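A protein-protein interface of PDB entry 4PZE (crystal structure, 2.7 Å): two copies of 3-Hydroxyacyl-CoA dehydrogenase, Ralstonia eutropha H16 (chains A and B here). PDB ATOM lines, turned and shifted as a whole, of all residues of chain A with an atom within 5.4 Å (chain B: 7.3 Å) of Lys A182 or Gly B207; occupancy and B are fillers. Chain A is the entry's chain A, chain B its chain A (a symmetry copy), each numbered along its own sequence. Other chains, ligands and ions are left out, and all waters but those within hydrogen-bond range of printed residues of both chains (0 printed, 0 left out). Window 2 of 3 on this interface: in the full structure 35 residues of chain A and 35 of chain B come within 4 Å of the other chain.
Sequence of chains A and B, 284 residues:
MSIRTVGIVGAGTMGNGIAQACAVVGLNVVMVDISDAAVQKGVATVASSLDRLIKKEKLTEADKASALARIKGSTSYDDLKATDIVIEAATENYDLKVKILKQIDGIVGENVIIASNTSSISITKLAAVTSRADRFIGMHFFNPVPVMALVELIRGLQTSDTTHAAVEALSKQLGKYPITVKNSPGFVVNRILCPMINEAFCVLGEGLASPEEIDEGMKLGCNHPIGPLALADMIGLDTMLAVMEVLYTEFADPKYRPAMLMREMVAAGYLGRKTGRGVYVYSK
O of Val B203 sits at hydrogen-bond distance from N of Leu B208.
N of Arg A155 is in hydrogen-bond range of O of Val A181, 2.9 Å away.
Among the printed residues, pairs that only touch across the chains: Lys A182 with Gly B207, Val A181 with Leu B208, Thr A180 with Ala B209, Ser A184 with Leu B208 and Thr A180 with Leu B208.
Gly B207 touches just one residue of chain A: Lys A182 (3.1 Å).
Of the printed residues of chain B, Val A181 touches Leu B208.
Of the printed residues of chain A, Ala B209 touches Thr A180 (3.3 Å).
Of the printed residues of chain B, Thr A180 touches Leu B208 (3.7 Å) and Ala B209 (3.3 Å).
Of the printed residues of chain B, Ser A184 touches Leu B208.
Glu B206 touches none of the printed residues of chain A.
Ile A154 touches none of the printed residues of chain B.
The nearest residue of chain B that does not touch Lys A182 is Ala B209 (5.3 Å).
Printed residues of chain A that touch a printed residue of chain B: Thr A180, Val A181, Lys A182 and Ser A184.
Hydrophobic or aromatic side chains of chain A that line the printed part of chain B: Val A181.
Of the 10 printed residues of chain B, 3 touch a printed residue of chain A.
No position is printed for both chains.
Of the 6 pairs that touch across the chains among the printed residues, none has its exchanged pair printed and touching as well.
The backbone carbonyl oxygen (O) of Leu B208 sits at hydrogen-bond distance from the backbone NH (N) of Lys A182 (3.0 Å).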
ATOM      1  N   ILE A 154       3.655 -11.087  -5.318  1.00  0.00           N
ATOM      2  CA  ILE A 154       2.358 -11.663  -5.550  1.00  0.00           C
ATOM      3  C   ILE A 154       1.404 -11.153  -4.488  1.00  0.00           C
ATOM      4  O   ILE A 154       1.570 -11.403  -3.278  1.00  0.00           O
ATOM      5  CB  ILE A 154       2.450 -13.179  -5.566  1.00  0.00           C
ATOM      6  CG1 ILE A 154       3.446 -13.617  -6.659  1.00  0.00           C
ATOM      7  CG2 ILE A 154       1.088 -13.782  -5.835  1.00  0.00           C
ATOM      8  CD1 ILE A 154       4.358 -14.757  -6.238  1.00  0.00           C
ATOM      9  N   ARG A 155       0.425 -10.380  -4.945  1.00  0.00           N
ATOM     10  CA  ARG A 155      -0.520  -9.782  -4.030  1.00  0.00           C
ATOM     11  C   ARG A 155      -1.609 -10.780  -3.760  1.00  0.00           C
ATOM     12  O   ARG A 155      -2.281 -11.228  -4.662  1.00  0.00           O
ATOM     13  CB  ARG A 155      -1.108  -8.506  -4.609  1.00  0.00           C
ATOM     14  CG  ARG A 155      -0.074  -7.412  -4.801  1.00  0.00           C
ATOM     15  CD  ARG A 155      -0.665  -6.133  -5.371  1.00  0.00           C
ATOM     16  NE  ARG A 155      -1.641  -5.510  -4.467  1.00  0.00           N
ATOM     17  CZ  ARG A 155      -2.044  -4.239  -4.513  1.00  0.00           C
ATOM     18  NH1 ARG A 155      -1.550  -3.376  -5.410  1.00  0.00           N
ATOM     19  NH2 ARG A 155      -2.922  -3.824  -3.615  1.00  0.00           N
ATOM     20  N   THR A 180       4.889  -7.741 -10.743  1.00  0.00           N
ATOM     21  CA  THR A 180       3.720  -7.755  -9.812  1.00  0.00           C
ATOM     22  C   THR A 180       2.559  -8.585 -10.394  1.00  0.00           C
ATOM     23  O   THR A 180       2.232  -8.487 -11.582  1.00  0.00           O
ATOM     24  CB  THR A 180       3.268  -6.333  -9.389  1.00  0.00           C
ATOM     25  OG1 THR A 180       3.922  -5.976  -8.164  1.00  0.00           O
ATOM     26  CG2 THR A 180       1.744  -6.230  -9.153  1.00  0.00           C
ATOM     27  N   VAL A 181       1.958  -9.427  -9.556  1.00  0.00           N
ATOM     28  CA  VAL A 181       1.053 -10.461 -10.055  1.00  0.00           C
ATOM     29  C   VAL A 181      -0.020 -10.603  -9.039  1.00  0.00           C
ATOM     30  O   VAL A 181       0.303 -10.702  -7.873  1.00  0.00           O
ATOM     31  CB  VAL A 181       1.739 -11.843 -10.201  1.00  0.00           C
ATOM     32  CG1 VAL A 181       0.852 -12.809 -10.951  1.00  0.00           C
ATOM     33  CG2 VAL A 181       3.062 -11.728 -10.948  1.00  0.00           C
ATOM     34  N   LYS A 182      -1.284 -10.607  -9.466  1.00  0.00           N
ATOM     35  CA  LYS A 182      -2.366 -10.958  -8.553  1.00  0.00           C
ATOM     36  C   LYS A 182      -2.269 -12.462  -8.312  1.00  0.00           C
ATOM     37  O   LYS A 182      -2.031 -13.228  -9.240  1.00  0.00           O
ATOM     38  CB  LYS A 182      -3.745 -10.643  -9.135  1.00  0.00           C
ATOM     39  CG  LYS A 182      -3.937  -9.204  -9.547  1.00  0.00           C
ATOM     40  CD  LYS A 182      -5.361  -8.950 -10.002  1.00  0.00           C
ATOM     41  CE  LYS A 182      -5.507  -7.542 -10.563  1.00  0.00           C
ATOM     42  NZ  LYS A 182      -6.887  -7.031 -10.320  1.00  0.00           N
ATOM     43  N   ASN A 183      -2.472 -12.883  -7.074  1.00  0.00           N
ATOM     44  CA  ASN A 183      -2.429 -14.304  -6.751  1.00  0.00           C
ATOM     45  C   ASN A 183      -3.251 -15.122  -7.744  1.00  0.00           C
ATOM     46  O   ASN A 183      -4.459 -14.903  -7.879  1.00  0.00           O
ATOM     47  CB  ASN A 183      -2.937 -14.550  -5.342  1.00  0.00           C
ATOM     48  CG  ASN A 183      -2.648 -15.946  -4.878  1.00  0.00           C
ATOM     49  OD1 ASN A 183      -1.481 -16.387  -4.849  1.00  0.00           O
ATOM     50  ND2 ASN A 183      -3.700 -16.668  -4.512  1.00  0.00           N
ATOM     51  N   SER A 184      -2.576 -16.021  -8.463  1.00  0.00           N
ATOM     52  CA  SER A 184      -3.225 -16.928  -9.429  1.00  0.00           C
ATOM     53  C   SER A 184      -2.363 -18.165  -9.604  1.00  0.00           C
ATOM     54  O   SER A 184      -1.123 -18.080  -9.576  1.00  0.00           O
ATOM     55  CB  SER A 184      -3.407 -16.243 -10.790  1.00  0.00           C
ATOM     56  OG  SER A 184      -3.424 -17.161 -11.882  1.00  0.00           O
ATOM     57  N   PHE A 187       1.266 -18.024 -10.948  1.00  0.00           N
ATOM     58  CA  PHE A 187       1.682 -16.634 -11.079  1.00  0.00           C
ATOM     59  C   PHE A 187       1.934 -16.297 -12.559  1.00  0.00           C
ATOM     60  O   PHE A 187       1.048 -16.514 -13.388  1.00  0.00           O
ATOM     61  CB  PHE A 187       2.869 -16.384 -10.140  1.00  0.00           C
ATOM     62  CG  PHE A 187       2.636 -16.910  -8.732  1.00  0.00           C
ATOM     63  CD1 PHE A 187       1.368 -16.862  -8.151  1.00  0.00           C
ATOM     64  CD2 PHE A 187       3.670 -17.442  -7.998  1.00  0.00           C
ATOM     65  CE1 PHE A 187       1.150 -17.345  -6.891  1.00  0.00           C
ATOM     66  CE2 PHE A 187       3.452 -17.927  -6.722  1.00  0.00           C
ATOM     67  CZ  PHE A 187       2.196 -17.873  -6.168  1.00  0.00           C
ATOM     68  N   PHE B 201      -1.125 -13.934 -23.636  1.00  0.00           N
ATOM     69  CA  PHE B 201      -2.371 -13.191 -23.858  1.00  0.00           C
ATOM     70  C   PHE B 201      -3.463 -13.558 -22.835  1.00  0.00           C
ATOM     71  O   PHE B 201      -4.203 -12.665 -22.376  1.00  0.00           O
ATOM     72  CB  PHE B 201      -2.865 -13.339 -25.315  1.00  0.00           C
ATOM     73  CG  PHE B 201      -2.040 -12.538 -26.308  1.00  0.00           C
ATOM     74  CD1 PHE B 201      -0.795 -12.983 -26.724  1.00  0.00           C
ATOM     75  CD2 PHE B 201      -2.491 -11.316 -26.790  1.00  0.00           C
ATOM     76  CE1 PHE B 201      -0.028 -12.246 -27.606  1.00  0.00           C
ATOM     77  CE2 PHE B 201      -1.725 -10.571 -27.673  1.00  0.00           C
ATOM     78  CZ  PHE B 201      -0.492 -11.039 -28.083  1.00  0.00           C
ATOM     79  N   CYS B 202      -3.569 -14.842 -22.463  1.00  0.00           N
ATOM     80  CA  CYS B 202      -4.552 -15.252 -21.444  1.00  0.00           C
ATOM     81  C   CYS B 202      -4.276 -14.568 -20.095  1.00  0.00           C
ATOM     82  O   CYS B 202      -5.206 -14.110 -19.399  1.00  0.00           O
ATOM     83  CB  CYS B 202      -4.588 -16.774 -21.259  1.00  0.00           C
ATOM     84  SG  CYS B 202      -5.379 -17.740 -22.576  1.00  0.00           S
ATOM     85  N   VAL B 203      -2.993 -14.504 -19.744  1.00  0.00           N
ATOM     86  CA  VAL B 203      -2.548 -13.931 -18.475  1.00  0.00           C
ATOM     87  C   VAL B 203      -2.825 -12.431 -18.422  1.00  0.00           C
ATOM     88  O   VAL B 203      -3.238 -11.906 -17.396  1.00  0.00           O
ATOM     89  CB  VAL B 203      -1.023 -14.188 -18.255  1.00  0.00           C
ATOM     90  CG1 VAL B 203      -0.490 -13.397 -17.084  1.00  0.00           C
ATOM     91  CG2 VAL B 203      -0.745 -15.663 -18.032  1.00  0.00           C
ATOM     92  N   LEU B 204      -2.550 -11.750 -19.532  1.00  0.00           N
ATOM     93  CA  LEU B 204      -2.756 -10.311 -19.679  1.00  0.00           C
ATOM     94  C   LEU B 204      -4.262 -10.006 -19.720  1.00  0.00           C
ATOM     95  O   LEU B 204      -4.746  -9.044 -19.117  1.00  0.00           O
ATOM     96  CB  LEU B 204      -2.073  -9.848 -20.973  1.00  0.00           C
ATOM     97  CG  LEU B 204      -2.299  -8.402 -21.420  1.00  0.00           C
ATOM     98  CD1 LEU B 204      -1.608  -7.462 -20.455  1.00  0.00           C
ATOM     99  CD2 LEU B 204      -1.788  -8.191 -22.830  1.00  0.00           C
ATOM    100  N   GLY B 205      -4.997 -10.848 -20.435  1.00  0.00           N
ATOM    101  CA  GLY B 205      -6.439 -10.752 -20.475  1.00  0.00           C
ATOM    102  C   GLY B 205      -7.036 -10.847 -19.102  1.00  0.00           C
ATOM    103  O   GLY B 205      -8.031 -10.213 -18.817  1.00  0.00           O
ATOM    104  N   GLU B 206      -6.423 -11.639 -18.232  1.00  0.00           N
ATOM    105  CA  GLU B 206      -7.028 -11.925 -16.924  1.00  0.00           C
ATOM    106  C   GLU B 206      -6.792 -10.804 -15.919  1.00  0.00           C
ATOM    107  O   GLU B 206      -7.297 -10.857 -14.802  1.00  0.00           O
ATOM    108  CB  GLU B 206      -6.548 -13.293 -16.367  1.00  0.00           C
ATOM    109  CG  GLU B 206      -7.226 -14.501 -17.015  1.00  0.00           C
ATOM    110  CD  GLU B 206      -6.416 -15.800 -16.928  1.00  0.00           C
ATOM    111  OE1 GLU B 206      -5.803 -16.065 -15.860  1.00  0.00           O
ATOM    112  OE2 GLU B 206      -6.386 -16.557 -17.935  1.00  0.00           O
ATOM    113  N   GLY B 207      -6.029  -9.796 -16.298  1.00  0.00           N
ATOM    114  CA  GLY B 207      -5.668  -8.737 -15.354  1.00  0.00           C
ATOM    115  C   GLY B 207      -4.571  -9.111 -14.362  1.00  0.00           C
ATOM    116  O   GLY B 207      -4.432  -8.472 -13.324  1.00  0.00           O
ATOM    117  N   LEU B 208      -3.780 -10.133 -14.652  1.00  0.00           N
ATOM    118  CA  LEU B 208      -2.863 -10.635 -13.617  1.00  0.00           C
ATOM    119  C   LEU B 208      -1.630  -9.797 -13.456  1.00  0.00           C
ATOM    120  O   LEU B 208      -1.137  -9.695 -12.348  1.00  0.00           O
ATOM    121  CB  LEU B 208      -2.467 -12.085 -13.856  1.00  0.00           C
ATOM    122  CG  LEU B 208      -3.700 -12.990 -13.851  1.00  0.00           C
ATOM    123  CD1 LEU B 208      -3.260 -14.386 -14.160  1.00  0.00           C
ATOM    124  CD2 LEU B 208      -4.470 -12.940 -12.541  1.00  0.00           C
ATOM    125  N   ALA B 209      -1.162  -9.181 -14.545  1.00  0.00           N
ATOM    126  CA  ALA B 209       0.102  -8.428 -14.583  1.00  0.00           C
ATOM    127  C   ALA B 209       0.170  -7.526 -15.831  1.00  0.00           C
ATOM    128  O   ALA B 209      -0.550  -7.733 -16.787  1.00  0.00           O
ATOM    129  CB  ALA B 209       1.279  -9.401 -14.578  1.00  0.00           C
ATOM    130  N   SER B 210       1.040  -6.532 -15.839  1.00  0.00           N
ATOM    131  CA  SER B 210       1.167  -5.656 -17.027  1.00  0.00           C
ATOM    132  C   SER B 210       1.912  -6.377 -18.170  1.00  0.00           C
ATOM    133  O   SER B 210       2.681  -7.314 -17.915  1.00  0.00           O
ATOM    134  CB  SER B 210       1.855  -4.325 -16.678  1.00  0.00           C
ATOM    135  OG  SER B 210       3.006  -4.533 -15.866  1.00  0.00           O
